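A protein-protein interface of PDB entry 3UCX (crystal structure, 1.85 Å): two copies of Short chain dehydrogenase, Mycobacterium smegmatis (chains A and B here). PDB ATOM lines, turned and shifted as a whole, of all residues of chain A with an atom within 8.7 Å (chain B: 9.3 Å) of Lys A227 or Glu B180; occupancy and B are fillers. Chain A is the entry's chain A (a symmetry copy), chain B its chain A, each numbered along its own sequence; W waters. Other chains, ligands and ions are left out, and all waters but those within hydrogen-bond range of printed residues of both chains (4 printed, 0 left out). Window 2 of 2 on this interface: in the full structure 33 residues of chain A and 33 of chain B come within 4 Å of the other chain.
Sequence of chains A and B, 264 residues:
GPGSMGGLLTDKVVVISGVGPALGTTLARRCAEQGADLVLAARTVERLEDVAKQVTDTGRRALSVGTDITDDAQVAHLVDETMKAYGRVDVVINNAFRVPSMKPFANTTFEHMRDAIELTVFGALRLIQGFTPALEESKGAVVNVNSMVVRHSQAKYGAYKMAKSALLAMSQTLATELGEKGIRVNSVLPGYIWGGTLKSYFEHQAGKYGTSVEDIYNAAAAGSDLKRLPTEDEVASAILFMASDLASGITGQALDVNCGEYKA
The side-chain carboxylate (OD1) of Asp A225 is in hydrogen-bond range of the side-chain hydroxyl (OG1) of Thr B176 (3.2 Å). The backbone carbonyl oxygen (O) of Asp A225 sits at hydrogen-bond distance from the backbone NH (N) of Glu B180 (3.4 Å). The backbone carbonyl oxygen (O) of Ser B248 lies within hydrogen-bond range of the guanidinium group (NH2) of Arg A228, 2.8 Å away. The backbone carbonyl oxygen of Asp A225 sits close to the backbone carbonyl oxygen of Gly B179 (3.3 Å).
The side-chain amino group of Lys A227 lies within hydrogen-bond range of the backbone carbonyl oxygen of Ala A222 (2.8 Å). The side-chain hydroxyl (OG) of Ser A224 is in hydrogen-bond range of the backbone NH (N) of Lys A227, 2.9 Å away. The backbone NH of Asp A225 is in hydrogen-bond range of the backbone carbonyl oxygen of Cys A259 (2.8 Å). The backbone NH of Leu A226 is in hydrogen-bond range of the backbone carbonyl oxygen of Cys A259. The backbone carbonyl oxygen of Arg A228 sits close to the side-chain sulfur of Cys A259, 3.4 Å away. The side-chain amide oxygen (OD1) of Asn A258 lies within hydrogen-bond range of the backbone NH (N) of Gly A260.
Asp A225 touches Ala B175 (CB to O, 3.4 Å). Thr B251 touches Asp A225 (CG2 to OD2, 3.6 Å). Gly B179 touches Leu A226. CD1 of Leu A226 touches CG2 of Thr B251, 3.9 Å away. CE of Lys A227 touches OE2 of Glu B180 (3.8 Å). Cys A259 touches Thr B251 (O to CG2, 3.4 Å). Gly A260 touches Thr B251.
Lys A227 touches just one residue of chain B: Glu B180 (3.8 Å). Glu B180 touches just these residues of chain A: Asp A225 and Lys A227. Gly A223 touches none of the printed residues of chain B. Gly B179 touches two residues of chain A. Printed residues of chain A within 4 Å of Thr B176: Asp A225. Printed residues of chain B within 4 Å of Cys A259: Thr B251 (3.4 Å). Of the printed residues of chain A, Thr B251 touches Asp A225, Leu A226, Cys A259 and Gly A260. Printed residues of chain A within 4 Å of Ala B175: Asp A225 (3.4 Å). Of the printed residues of chain B, Leu A226 touches Gly B179 and Thr B251. Val B185 touches none of the printed residues of chain A. Leu B174 touches none of the printed residues of chain A. The nearest residue of chain B that does not touch Lys A227 is Gly B179 (5.3 Å). The nearest residue of chain A that does not touch Glu B180 is Leu A226 (5.2 Å).
Of the 18 printed residues of chain B, 6 touch a printed residue of chain A.
No position is printed for both chains.
Water W1 bridges O of Gly B182 (2.7 Å) and NH2 of Arg A228 (3.1 Å). Water W3 bridges the backbone carbonyl oxygen (O) of Thr B176 (2.7 Å) and the backbone carbonyl oxygen (O) of Asp A225 (2.7 Å). Water W2 bridges the backbone carbonyl oxygen (O) of Leu A226 (2.8 Å) and the backbone carbonyl oxygen (O) of Gly B179 (2.9 Å). Water W4 lies within hydrogen-bond range of the side-chain amide oxygen (OD1) of Asn A258 and the backbone NH (N) of Thr B251.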
ATOM      1  N   TYR A 217       5.382 -13.558 -20.351  1.00  0.00           N
ATOM      2  CA  TYR A 217       6.747 -13.393 -20.857  1.00  0.00           C
ATOM      3  C   TYR A 217       7.203 -11.958 -20.679  1.00  0.00           C
ATOM      4  O   TYR A 217       8.283 -11.701 -20.134  1.00  0.00           O
ATOM      5  CB  TYR A 217       6.879 -13.817 -22.326  1.00  0.00           C
ATOM      6  CG  TYR A 217       8.276 -13.651 -22.901  1.00  0.00           C
ATOM      7  CD1 TYR A 217       8.742 -12.400 -23.332  1.00  0.00           C
ATOM      8  CD2 TYR A 217       9.121 -14.738 -23.039  1.00  0.00           C
ATOM      9  CE1 TYR A 217      10.008 -12.247 -23.874  1.00  0.00           C
ATOM     10  CE2 TYR A 217      10.405 -14.595 -23.555  1.00  0.00           C
ATOM     11  CZ  TYR A 217      10.844 -13.347 -23.972  1.00  0.00           C
ATOM     12  OH  TYR A 217      12.103 -13.206 -24.505  1.00  0.00           O
ATOM     13  N   ASN A 218       6.399 -11.005 -21.130  1.00  0.00           N
ATOM     14  CA  ASN A 218       6.793  -9.602 -21.043  1.00  0.00           C
ATOM     15  C   ASN A 218       6.980  -9.164 -19.580  1.00  0.00           C
ATOM     16  O   ASN A 218       7.915  -8.423 -19.281  1.00  0.00           O
ATOM     17  CB  ASN A 218       5.771  -8.685 -21.754  1.00  0.00           C
ATOM     18  CG  ASN A 218       5.736  -8.884 -23.263  1.00  0.00           C
ATOM     19  OD1 ASN A 218       6.736  -9.237 -23.896  1.00  0.00           O
ATOM     20  ND2 ASN A 218       4.573  -8.616 -23.858  1.00  0.00           N
ATOM     21  N   ALA A 219       6.119  -9.623 -18.667  1.00  0.00           N
ATOM     22  CA  ALA A 219       6.308  -9.322 -17.245  1.00  0.00           C
ATOM     23  C   ALA A 219       7.638  -9.896 -16.733  1.00  0.00           C
ATOM     24  O   ALA A 219       8.366  -9.218 -16.005  1.00  0.00           O
ATOM     25  CB  ALA A 219       5.123  -9.795 -16.371  1.00  0.00           C
ATOM     26  N   ALA A 220       7.962 -11.117 -17.128  1.00  0.00           N
ATOM     27  CA  ALA A 220       9.195 -11.750 -16.700  1.00  0.00           C
ATOM     28  C   ALA A 220      10.419 -10.992 -17.247  1.00  0.00           C
ATOM     29  O   ALA A 220      11.444 -10.868 -16.553  1.00  0.00           O
ATOM     30  CB  ALA A 220       9.227 -13.200 -17.151  1.00  0.00           C
ATOM     31  N   ALA A 221      10.311 -10.488 -18.482  1.00  0.00           N
ATOM     32  CA  ALA A 221      11.431  -9.819 -19.163  1.00  0.00           C
ATOM     33  C   ALA A 221      11.562  -8.318 -18.887  1.00  0.00           C
ATOM     34  O   ALA A 221      12.550  -7.690 -19.305  1.00  0.00           O
ATOM     35  CB  ALA A 221      11.345 -10.077 -20.662  1.00  0.00           C
ATOM     36  N   ALA A 222      10.591  -7.743 -18.161  1.00  0.00           N
ATOM     37  CA  ALA A 222      10.470  -6.281 -18.043  1.00  0.00           C
ATOM     38  C   ALA A 222      11.637  -5.665 -17.296  1.00  0.00           C
ATOM     39  O   ALA A 222      12.033  -4.561 -17.595  1.00  0.00           O
ATOM     40  CB  ALA A 222       9.133  -5.889 -17.369  1.00  0.00           C
ATOM     41  N   GLY A 223      12.201  -6.383 -16.332  1.00  0.00           N
ATOM     42  CA  GLY A 223      13.323  -5.852 -15.551  1.00  0.00           C
ATOM     43  C   GLY A 223      14.646  -5.888 -16.313  1.00  0.00           C
ATOM     44  O   GLY A 223      15.613  -5.222 -15.914  1.00  0.00           O
ATOM     45  N   SER A 224      14.706  -6.659 -17.392  1.00  0.00           N
ATOM     46  CA  SER A 224      15.958  -6.807 -18.156  1.00  0.00           C
ATOM     47  C   SER A 224      16.225  -5.547 -18.973  1.00  0.00           C
ATOM     48  O   SER A 224      15.298  -4.767 -19.244  1.00  0.00           O
ATOM     49  CB  SER A 224      15.917  -8.023 -19.083  1.00  0.00           C
ATOM     50  OG  SER A 224      15.041  -7.832 -20.193  1.00  0.00           O
ATOM     51  N   ASP A 225      17.485  -5.355 -19.366  1.00  0.00           N
ATOM     52  CA  ASP A 225      17.844  -4.237 -20.245  1.00  0.00           C
ATOM     53  C   ASP A 225      17.359  -4.448 -21.681  1.00  0.00           C
ATOM     54  O   ASP A 225      17.019  -3.496 -22.384  1.00  0.00           O
ATOM     55  CB  ASP A 225      19.360  -4.050 -20.297  1.00  0.00           C
ATOM     56  CG  ASP A 225      19.960  -3.666 -18.945  1.00  0.00           C
ATOM     57  OD1 ASP A 225      19.267  -3.067 -18.080  1.00  0.00           O
ATOM     58  OD2 ASP A 225      21.148  -3.963 -18.780  1.00  0.00           O
ATOM     59  N   LEU A 226      17.407  -5.694 -22.125  1.00  0.00           N
ATOM     60  CA  LEU A 226      17.150  -6.044 -23.521  1.00  0.00           C
ATOM     61  C   LEU A 226      15.681  -6.350 -23.808  1.00  0.00           C
ATOM     62  O   LEU A 226      15.272  -6.482 -24.967  1.00  0.00           O
ATOM     63  CB  LEU A 226      18.048  -7.209 -23.919  1.00  0.00           C
ATOM     64  CG  LEU A 226      19.549  -6.905 -23.861  1.00  0.00           C
ATOM     65  CD1 LEU A 226      20.339  -8.208 -23.952  1.00  0.00           C
ATOM     66  CD2 LEU A 226      20.017  -5.948 -24.943  1.00  0.00           C
ATOM     67  N   LYS A 227      14.896  -6.466 -22.746  1.00  0.00           N
ATOM     68  CA  LYS A 227      13.471  -6.787 -22.814  1.00  0.00           C
ATOM     69  C   LYS A 227      13.233  -8.115 -23.504  1.00  0.00           C
ATOM     70  O   LYS A 227      12.284  -8.278 -24.277  1.00  0.00           O
ATOM     71  CB  LYS A 227      12.697  -5.665 -23.500  1.00  0.00           C
ATOM     72  CG  LYS A 227      13.018  -4.291 -22.951  1.00  0.00           C
ATOM     73  CD  LYS A 227      12.714  -4.187 -21.473  1.00  0.00           C
ATOM     74  CE  LYS A 227      13.274  -2.886 -20.940  1.00  0.00           C
ATOM     75  NZ  LYS A 227      13.145  -2.780 -19.469  1.00  0.00           N
ATOM     76  N   ARG A 228      14.124  -9.065 -23.212  1.00  0.00           N
ATOM     77  CA  ARG A 228      13.953 -10.457 -23.634  1.00  0.00           C
ATOM     78  C   ARG A 228      14.588 -11.340 -22.577  1.00  0.00           C
ATOM     79  O   ARG A 228      15.469 -10.897 -21.840  1.00  0.00           O
ATOM     80  CB  ARG A 228      14.601 -10.740 -24.994  1.00  0.00           C
ATOM     81  CG  ARG A 228      16.025 -10.272 -25.191  1.00  0.00           C
ATOM     82  CD  ARG A 228      16.507 -10.543 -26.610  1.00  0.00           C
ATOM     83  NE  ARG A 228      17.825  -9.929 -26.924  1.00  0.00           N
ATOM     84  CZ  ARG A 228      19.010 -10.523 -26.731  1.00  0.00           C
ATOM     85  NH1 ARG A 228      19.080 -11.728 -26.195  1.00  0.00           N
ATOM     86  NH2 ARG A 228      20.138  -9.909 -27.075  1.00  0.00           N
ATOM     87  N   LEU A 229      14.117 -12.574 -22.488  1.00  0.00           N
ATOM     88  CA  LEU A 229      14.718 -13.551 -21.591  1.00  0.00           C
ATOM     89  C   LEU A 229      15.863 -14.229 -22.342  1.00  0.00           C
ATOM     90  O   LEU A 229      15.771 -14.449 -23.562  1.00  0.00           O
ATOM     91  CB  LEU A 229      13.666 -14.591 -21.188  1.00  0.00           C
ATOM     92  CG  LEU A 229      12.470 -14.102 -20.374  1.00  0.00           C
ATOM     93  CD1 LEU A 229      11.571 -15.286 -20.037  1.00  0.00           C
ATOM     94  CD2 LEU A 229      12.926 -13.403 -19.085  1.00  0.00           C
ATOM     95  N   PRO A 230      16.954 -14.584 -21.626  1.00  0.00           N
ATOM     96  CA  PRO A 230      17.965 -15.384 -22.278  1.00  0.00           C
ATOM     97  C   PRO A 230      17.421 -16.757 -22.653  1.00  0.00           C
ATOM     98  O   PRO A 230      16.535 -17.279 -21.977  1.00  0.00           O
ATOM     99  CB  PRO A 230      19.081 -15.491 -21.223  1.00  0.00           C
ATOM    100  CG  PRO A 230      18.381 -15.355 -19.951  1.00  0.00           C
ATOM    101  CD  PRO A 230      17.232 -14.397 -20.198  1.00  0.00           C
ATOM    102  N   ASN A 258      21.401 -12.848 -17.882  1.00  0.00           N
ATOM    103  CA  ASN A 258      20.087 -12.378 -17.508  1.00  0.00           C
ATOM    104  C   ASN A 258      19.588 -11.187 -18.284  1.00  0.00           C
ATOM    105  O   ASN A 258      18.628 -10.526 -17.856  1.00  0.00           O
ATOM    106  CB  ASN A 258      20.065 -12.083 -15.993  1.00  0.00           C
ATOM    107  CG  ASN A 258      21.033 -10.995 -15.576  1.00  0.00           C
ATOM    108  OD1 ASN A 258      21.406 -10.127 -16.372  1.00  0.00           O
ATOM    109  ND2 ASN A 258      21.432 -11.010 -14.288  1.00  0.00           N
ATOM    110  N   CYS A 259      20.222 -10.908 -19.415  1.00  0.00           N
ATOM    111  CA  CYS A 259      19.839  -9.806 -20.288  1.00  0.00           C
ATOM    112  C   CYS A 259      19.838  -8.463 -19.570  1.00  0.00           C
ATOM    113  O   CYS A 259      19.183  -7.517 -20.005  1.00  0.00           O
ATOM    114  CB  CYS A 259      18.513 -10.119 -21.008  1.00  0.00           C
ATOM    115  SG  CYS A 259      18.768 -11.481 -22.153  1.00  0.00           S
ATOM    116  N   GLY A 260      20.633  -8.386 -18.492  1.00  0.00           N
ATOM    117  CA  GLY A 260      20.851  -7.134 -17.782  1.00  0.00           C
ATOM    118  C   GLY A 260      19.994  -6.878 -16.552  1.00  0.00           C
ATOM    119  O   GLY A 260      20.163  -5.856 -15.925  1.00  0.00           O
ATOM    120  N   GLU A 261      19.127  -7.801 -16.164  1.00  0.00           N
ATOM    121  CA  GLU A 261      18.204  -7.541 -15.056  1.00  0.00           C
ATOM    122  C   GLU A 261      18.912  -7.187 -13.744  1.00  0.00           C
ATOM    123  O   GLU A 261      18.505  -6.248 -13.038  1.00  0.00           O
ATOM    124  CB  GLU A 261      17.217  -8.701 -14.858  1.00  0.00           C
ATOM    125  CG  GLU A 261      16.108  -8.326 -13.885  1.00  0.00           C
ATOM    126  CD  GLU A 261      14.938  -9.278 -13.840  1.00  0.00           C
ATOM    127  OE1 GLU A 261      14.925 -10.307 -14.507  1.00  0.00           O
ATOM    128  OE2 GLU A 261      14.013  -8.997 -13.066  1.00  0.00           O
ATOM    129  N   LEU B 135      25.829   0.964 -33.974  1.00  0.00           N
ATOM    130  CA  LEU B 135      25.486  -0.156 -33.096  1.00  0.00           C
ATOM    131  C   LEU B 135      24.000  -0.433 -33.004  1.00  0.00           C
ATOM    132  O   LEU B 135      23.614  -1.595 -32.825  1.00  0.00           O
ATOM    133  CB  LEU B 135      26.059   0.080 -31.702  1.00  0.00           C
ATOM    134  CG  LEU B 135      27.582   0.058 -31.649  1.00  0.00           C
ATOM    135  CD1 LEU B 135      28.025   0.602 -30.300  1.00  0.00           C
ATOM    136  CD2 LEU B 135      28.137  -1.337 -31.907  1.00  0.00           C
ATOM    137  N   GLU B 136      23.159   0.595 -33.167  1.00  0.00           N
ATOM    138  CA  GLU B 136      21.706   0.391 -33.195  1.00  0.00           C
ATOM    139  C   GLU B 136      21.335  -0.488 -34.376  1.00  0.00           C
ATOM    140  O   GLU B 136      20.513  -1.399 -34.237  1.00  0.00           O
ATOM    141  CB  GLU B 136      20.883   1.697 -33.316  1.00  0.00           C
ATOM    142  CG  GLU B 136      20.994   2.655 -32.168  1.00  0.00           C
ATOM    143  CD  GLU B 136      20.104   3.893 -32.318  1.00  0.00           C
ATOM    144  OE1 GLU B 136      19.320   3.953 -33.260  1.00  0.00           O
ATOM    145  OE2 GLU B 136      20.204   4.818 -31.492  1.00  0.00           O
ATOM    146  N   LYS B 139      22.616  -4.080 -33.874  1.00  0.00           N
ATOM    147  CA  LYS B 139      22.353  -4.663 -32.553  1.00  0.00           C
ATOM    148  C   LYS B 139      23.669  -5.171 -31.960  1.00  0.00           C
ATOM    149  O   LYS B 139      23.804  -6.339 -31.544  1.00  0.00           O
ATOM    150  CB  LYS B 139      21.297  -5.788 -32.633  1.00  0.00           C
ATOM    151  N   THR B 173      24.952   1.779 -16.359  1.00  0.00           N
ATOM    152  CA  THR B 173      23.829   2.611 -16.808  1.00  0.00           C
ATOM    153  C   THR B 173      23.640   2.513 -18.344  1.00  0.00           C
ATOM    154  O   THR B 173      22.498   2.449 -18.842  1.00  0.00           O
ATOM    155  CB  THR B 173      24.047   4.081 -16.421  1.00  0.00           C
ATOM    156  OG1 THR B 173      24.209   4.186 -14.988  1.00  0.00           O
ATOM    157  CG2 THR B 173      22.829   4.961 -16.875  1.00  0.00           C
ATOM    158  N   LEU B 174      24.755   2.470 -19.079  1.00  0.00           N
ATOM    159  CA  LEU B 174      24.690   2.378 -20.538  1.00  0.00           C
ATOM    160  C   LEU B 174      24.059   1.073 -20.979  1.00  0.00           C
ATOM    161  O   LEU B 174      23.385   1.035 -22.020  1.00  0.00           O
ATOM    162  CB  LEU B 174      26.055   2.585 -21.208  1.00  0.00           C
ATOM    163  CG  LEU B 174      26.581   4.035 -21.258  1.00  0.00           C
ATOM    164  CD1 LEU B 174      28.033   4.093 -21.770  1.00  0.00           C
ATOM    165  CD2 LEU B 174      25.663   4.918 -22.146  1.00  0.00           C
ATOM    166  N   ALA B 175      24.283  -0.013 -20.233  1.00  0.00           N
ATOM    167  CA  ALA B 175      23.616  -1.269 -20.557  1.00  0.00           C
ATOM    168  C   ALA B 175      22.087  -1.069 -20.476  1.00  0.00           C
ATOM    169  O   ALA B 175      21.333  -1.522 -21.357  1.00  0.00           O
ATOM    170  CB  ALA B 175      24.080  -2.400 -19.621  1.00  0.00           C
ATOM    171  N   THR B 176      21.631  -0.366 -19.445  1.00  0.00           N
ATOM    172  CA  THR B 176      20.207  -0.098 -19.298  1.00  0.00           C
ATOM    173  C   THR B 176      19.727   0.779 -20.450  1.00  0.00           C
ATOM    174  O   THR B 176      18.712   0.455 -21.108  1.00  0.00           O
ATOM    175  CB  THR B 176      19.898   0.565 -17.952  1.00  0.00           C
ATOM    176  OG1 THR B 176      20.388  -0.286 -16.920  1.00  0.00           O
ATOM    177  CG2 THR B 176      18.375   0.804 -17.762  1.00  0.00           C
ATOM    178  N   GLU B 177      20.441   1.876 -20.683  1.00  0.00           N
ATOM    179  CA  GLU B 177      19.988   2.890 -21.622  1.00  0.00           C
ATOM    180  C   GLU B 177      20.077   2.470 -23.085  1.00  0.00           C
ATOM    181  O   GLU B 177      19.253   2.887 -23.902  1.00  0.00           O
ATOM    182  CB  GLU B 177      20.709   4.212 -21.370  1.00  0.00           C
ATOM    183  CG  GLU B 177      20.308   4.803 -20.019  1.00  0.00           C
ATOM    184  CD  GLU B 177      20.871   6.184 -19.732  1.00  0.00           C
ATOM    185  OE1 GLU B 177      21.741   6.667 -20.494  1.00  0.00           O
ATOM    186  OE2 GLU B 177      20.452   6.763 -18.683  1.00  0.00           O
ATOM    187  N   LEU B 178      21.070   1.679 -23.441  1.00  0.00           N
ATOM    188  CA  LEU B 178      21.222   1.239 -24.799  1.00  0.00           C
ATOM    189  C   LEU B 178      20.558  -0.124 -25.046  1.00  0.00           C
ATOM    190  O   LEU B 178      20.362  -0.491 -26.188  1.00  0.00           O
ATOM    191  CB  LEU B 178      22.689   1.216 -25.203  1.00  0.00           C
ATOM    192  CG  LEU B 178      23.496   2.504 -25.049  1.00  0.00           C
ATOM    193  CD1 LEU B 178      24.936   2.285 -25.500  1.00  0.00           C
ATOM    194  CD2 LEU B 178      22.818   3.627 -25.855  1.00  0.00           C
ATOM    195  N   GLY B 179      20.196  -0.845 -23.976  1.00  0.00           N
ATOM    196  CA  GLY B 179      19.552  -2.152 -24.095  1.00  0.00           C
ATOM    197  C   GLY B 179      18.227  -2.131 -24.863  1.00  0.00           C
ATOM    198  O   GLY B 179      17.902  -3.066 -25.562  1.00  0.00           O
ATOM    199  N   GLU B 180      17.476  -1.054 -24.774  1.00  0.00           N
ATOM    200  CA  GLU B 180      16.235  -0.996 -25.549  1.00  0.00           C
ATOM    201  C   GLU B 180      16.456  -0.894 -27.053  1.00  0.00           C
ATOM    202  O   GLU B 180      15.591  -1.308 -27.831  1.00  0.00           O
ATOM    203  CB  GLU B 180      15.287   0.093 -25.047  1.00  0.00           C
ATOM    204  CG  GLU B 180      14.162  -0.540 -24.233  1.00  0.00           C
ATOM    205  CD  GLU B 180      13.136   0.464 -23.751  1.00  0.00           C
ATOM    206  OE1 GLU B 180      13.287   1.675 -24.055  1.00  0.00           O
ATOM    207  OE2 GLU B 180      12.183   0.032 -23.067  1.00  0.00           O
ATOM    208  N   LYS B 181      17.637  -0.445 -27.456  1.00  0.00           N
ATOM    209  CA  LYS B 181      18.038  -0.497 -28.856  1.00  0.00           C
ATOM    210  C   LYS B 181      18.697  -1.826 -29.256  1.00  0.00           C
ATOM    211  O   LYS B 181      19.117  -1.984 -30.392  1.00  0.00           O
ATOM    212  CB  LYS B 181      19.015   0.614 -29.119  1.00  0.00           C
ATOM    213  CG  LYS B 181      18.460   1.988 -28.860  1.00  0.00           C
ATOM    214  CD  LYS B 181      19.632   2.917 -29.073  1.00  0.00           C
ATOM    215  CE  LYS B 181      19.589   4.158 -28.239  1.00  0.00           C
ATOM    216  NZ  LYS B 181      19.139   5.237 -29.097  1.00  0.00           N
ATOM    217  N   GLY B 182      18.784  -2.765 -28.317  1.00  0.00           N
ATOM    218  CA  GLY B 182      19.366  -4.070 -28.558  1.00  0.00           C
ATOM    219  C   GLY B 182      20.882  -4.064 -28.499  1.00  0.00           C
ATOM    220  O   GLY B 182      21.502  -5.027 -28.961  1.00  0.00           O
ATOM    221  N   ILE B 183      21.482  -3.004 -27.946  1.00  0.00           N
ATOM    222  CA  ILE B 183      22.948  -2.890 -27.850  1.00  0.00           C
ATOM    223  C   ILE B 183      23.376  -3.437 -26.471  1.00  0.00           C
ATOM    224  O   ILE B 183      22.840  -3.005 -25.463  1.00  0.00           O
ATOM    225  CB  ILE B 183      23.436  -1.433 -27.993  1.00  0.00           C
ATOM    226  CG1 ILE B 183      23.059  -0.860 -29.383  1.00  0.00           C
ATOM    227  CG2 ILE B 183      24.938  -1.306 -27.774  1.00  0.00           C
ATOM    228  CD1 ILE B 183      23.191   0.655 -29.422  1.00  0.00           C
ATOM    229  N   ARG B 184      24.319  -4.375 -26.472  1.00  0.00           N
ATOM    230  CA  ARG B 184      24.892  -4.944 -25.245  1.00  0.00           C
ATOM    231  C   ARG B 184      26.104  -4.132 -24.809  1.00  0.00           C
ATOM    232  O   ARG B 184      26.873  -3.623 -25.640  1.00  0.00           O
ATOM    233  CB  ARG B 184      25.283  -6.408 -25.453  1.00  0.00           C
ATOM    234  CG  ARG B 184      24.095  -7.283 -25.813  1.00  0.00           C
ATOM    235  CD  ARG B 184      24.426  -8.769 -25.898  1.00  0.00           C
ATOM    236  NE  ARG B 184      25.485  -9.054 -26.860  1.00  0.00           N
ATOM    237  CZ  ARG B 184      26.785  -9.267 -26.571  1.00  0.00           C
ATOM    238  NH1 ARG B 184      27.269  -9.280 -25.330  1.00  0.00           N
ATOM    239  NH2 ARG B 184      27.616  -9.506 -27.566  1.00  0.00           N
ATOM    240  N   VAL B 185      26.276  -3.999 -23.498  1.00  0.00           N
ATOM    241  CA  VAL B 185      27.420  -3.291 -22.937  1.00  0.00           C
ATOM    242  C   VAL B 185      27.929  -4.081 -21.743  1.00  0.00           C
ATOM    243  O   VAL B 185      27.226  -4.264 -20.757  1.00  0.00           O
ATOM    244  CB  VAL B 185      27.074  -1.870 -22.470  1.00  0.00           C
ATOM    245  CG1 VAL B 185      28.337  -1.146 -21.964  1.00  0.00           C
ATOM    246  CG2 VAL B 185      26.359  -1.071 -23.587  1.00  0.00           C
ATOM    247  N   SER B 248      25.236 -13.206 -26.379  1.00  0.00           N
ATOM    248  CA  SER B 248      24.024 -12.433 -26.756  1.00  0.00           C
ATOM    249  C   SER B 248      22.971 -12.315 -25.642  1.00  0.00           C
ATOM    250  O   SER B 248      22.079 -11.443 -25.706  1.00  0.00           O
ATOM    251  CB  SER B 248      23.412 -12.951 -28.077  1.00  0.00           C
ATOM    252  OG  SER B 248      23.010 -14.298 -27.944  1.00  0.00           O
ATOM    253  N   THR B 251      24.381  -8.761 -20.774  1.00  0.00           N
ATOM    254  CA  THR B 251      24.677  -7.338 -20.780  1.00  0.00           C
ATOM    255  C   THR B 251      24.668  -6.825 -19.355  1.00  0.00           C
ATOM    256  O   THR B 251      24.035  -7.407 -18.478  1.00  0.00           O
ATOM    257  CB  THR B 251      23.694  -6.549 -21.671  1.00  0.00           C
ATOM    258  OG1 THR B 251      24.203  -5.226 -21.912  1.00  0.00           O
ATOM    259  CG2 THR B 251      22.293  -6.487 -21.012  1.00  0.00           C
HETATM  260  O   HOH W   1      20.554  -7.524 -29.027  1.00  0.00           O
HETATM  261  O   HOH W   2      16.639  -5.262 -27.045  1.00  0.00           O
HETATM  262  O   HOH W   3      16.493  -1.128 -21.114  1.00  0.00           O
HETATM  263  O   HOH W   4      23.566 -10.859 -18.135  1.00  0.00           O
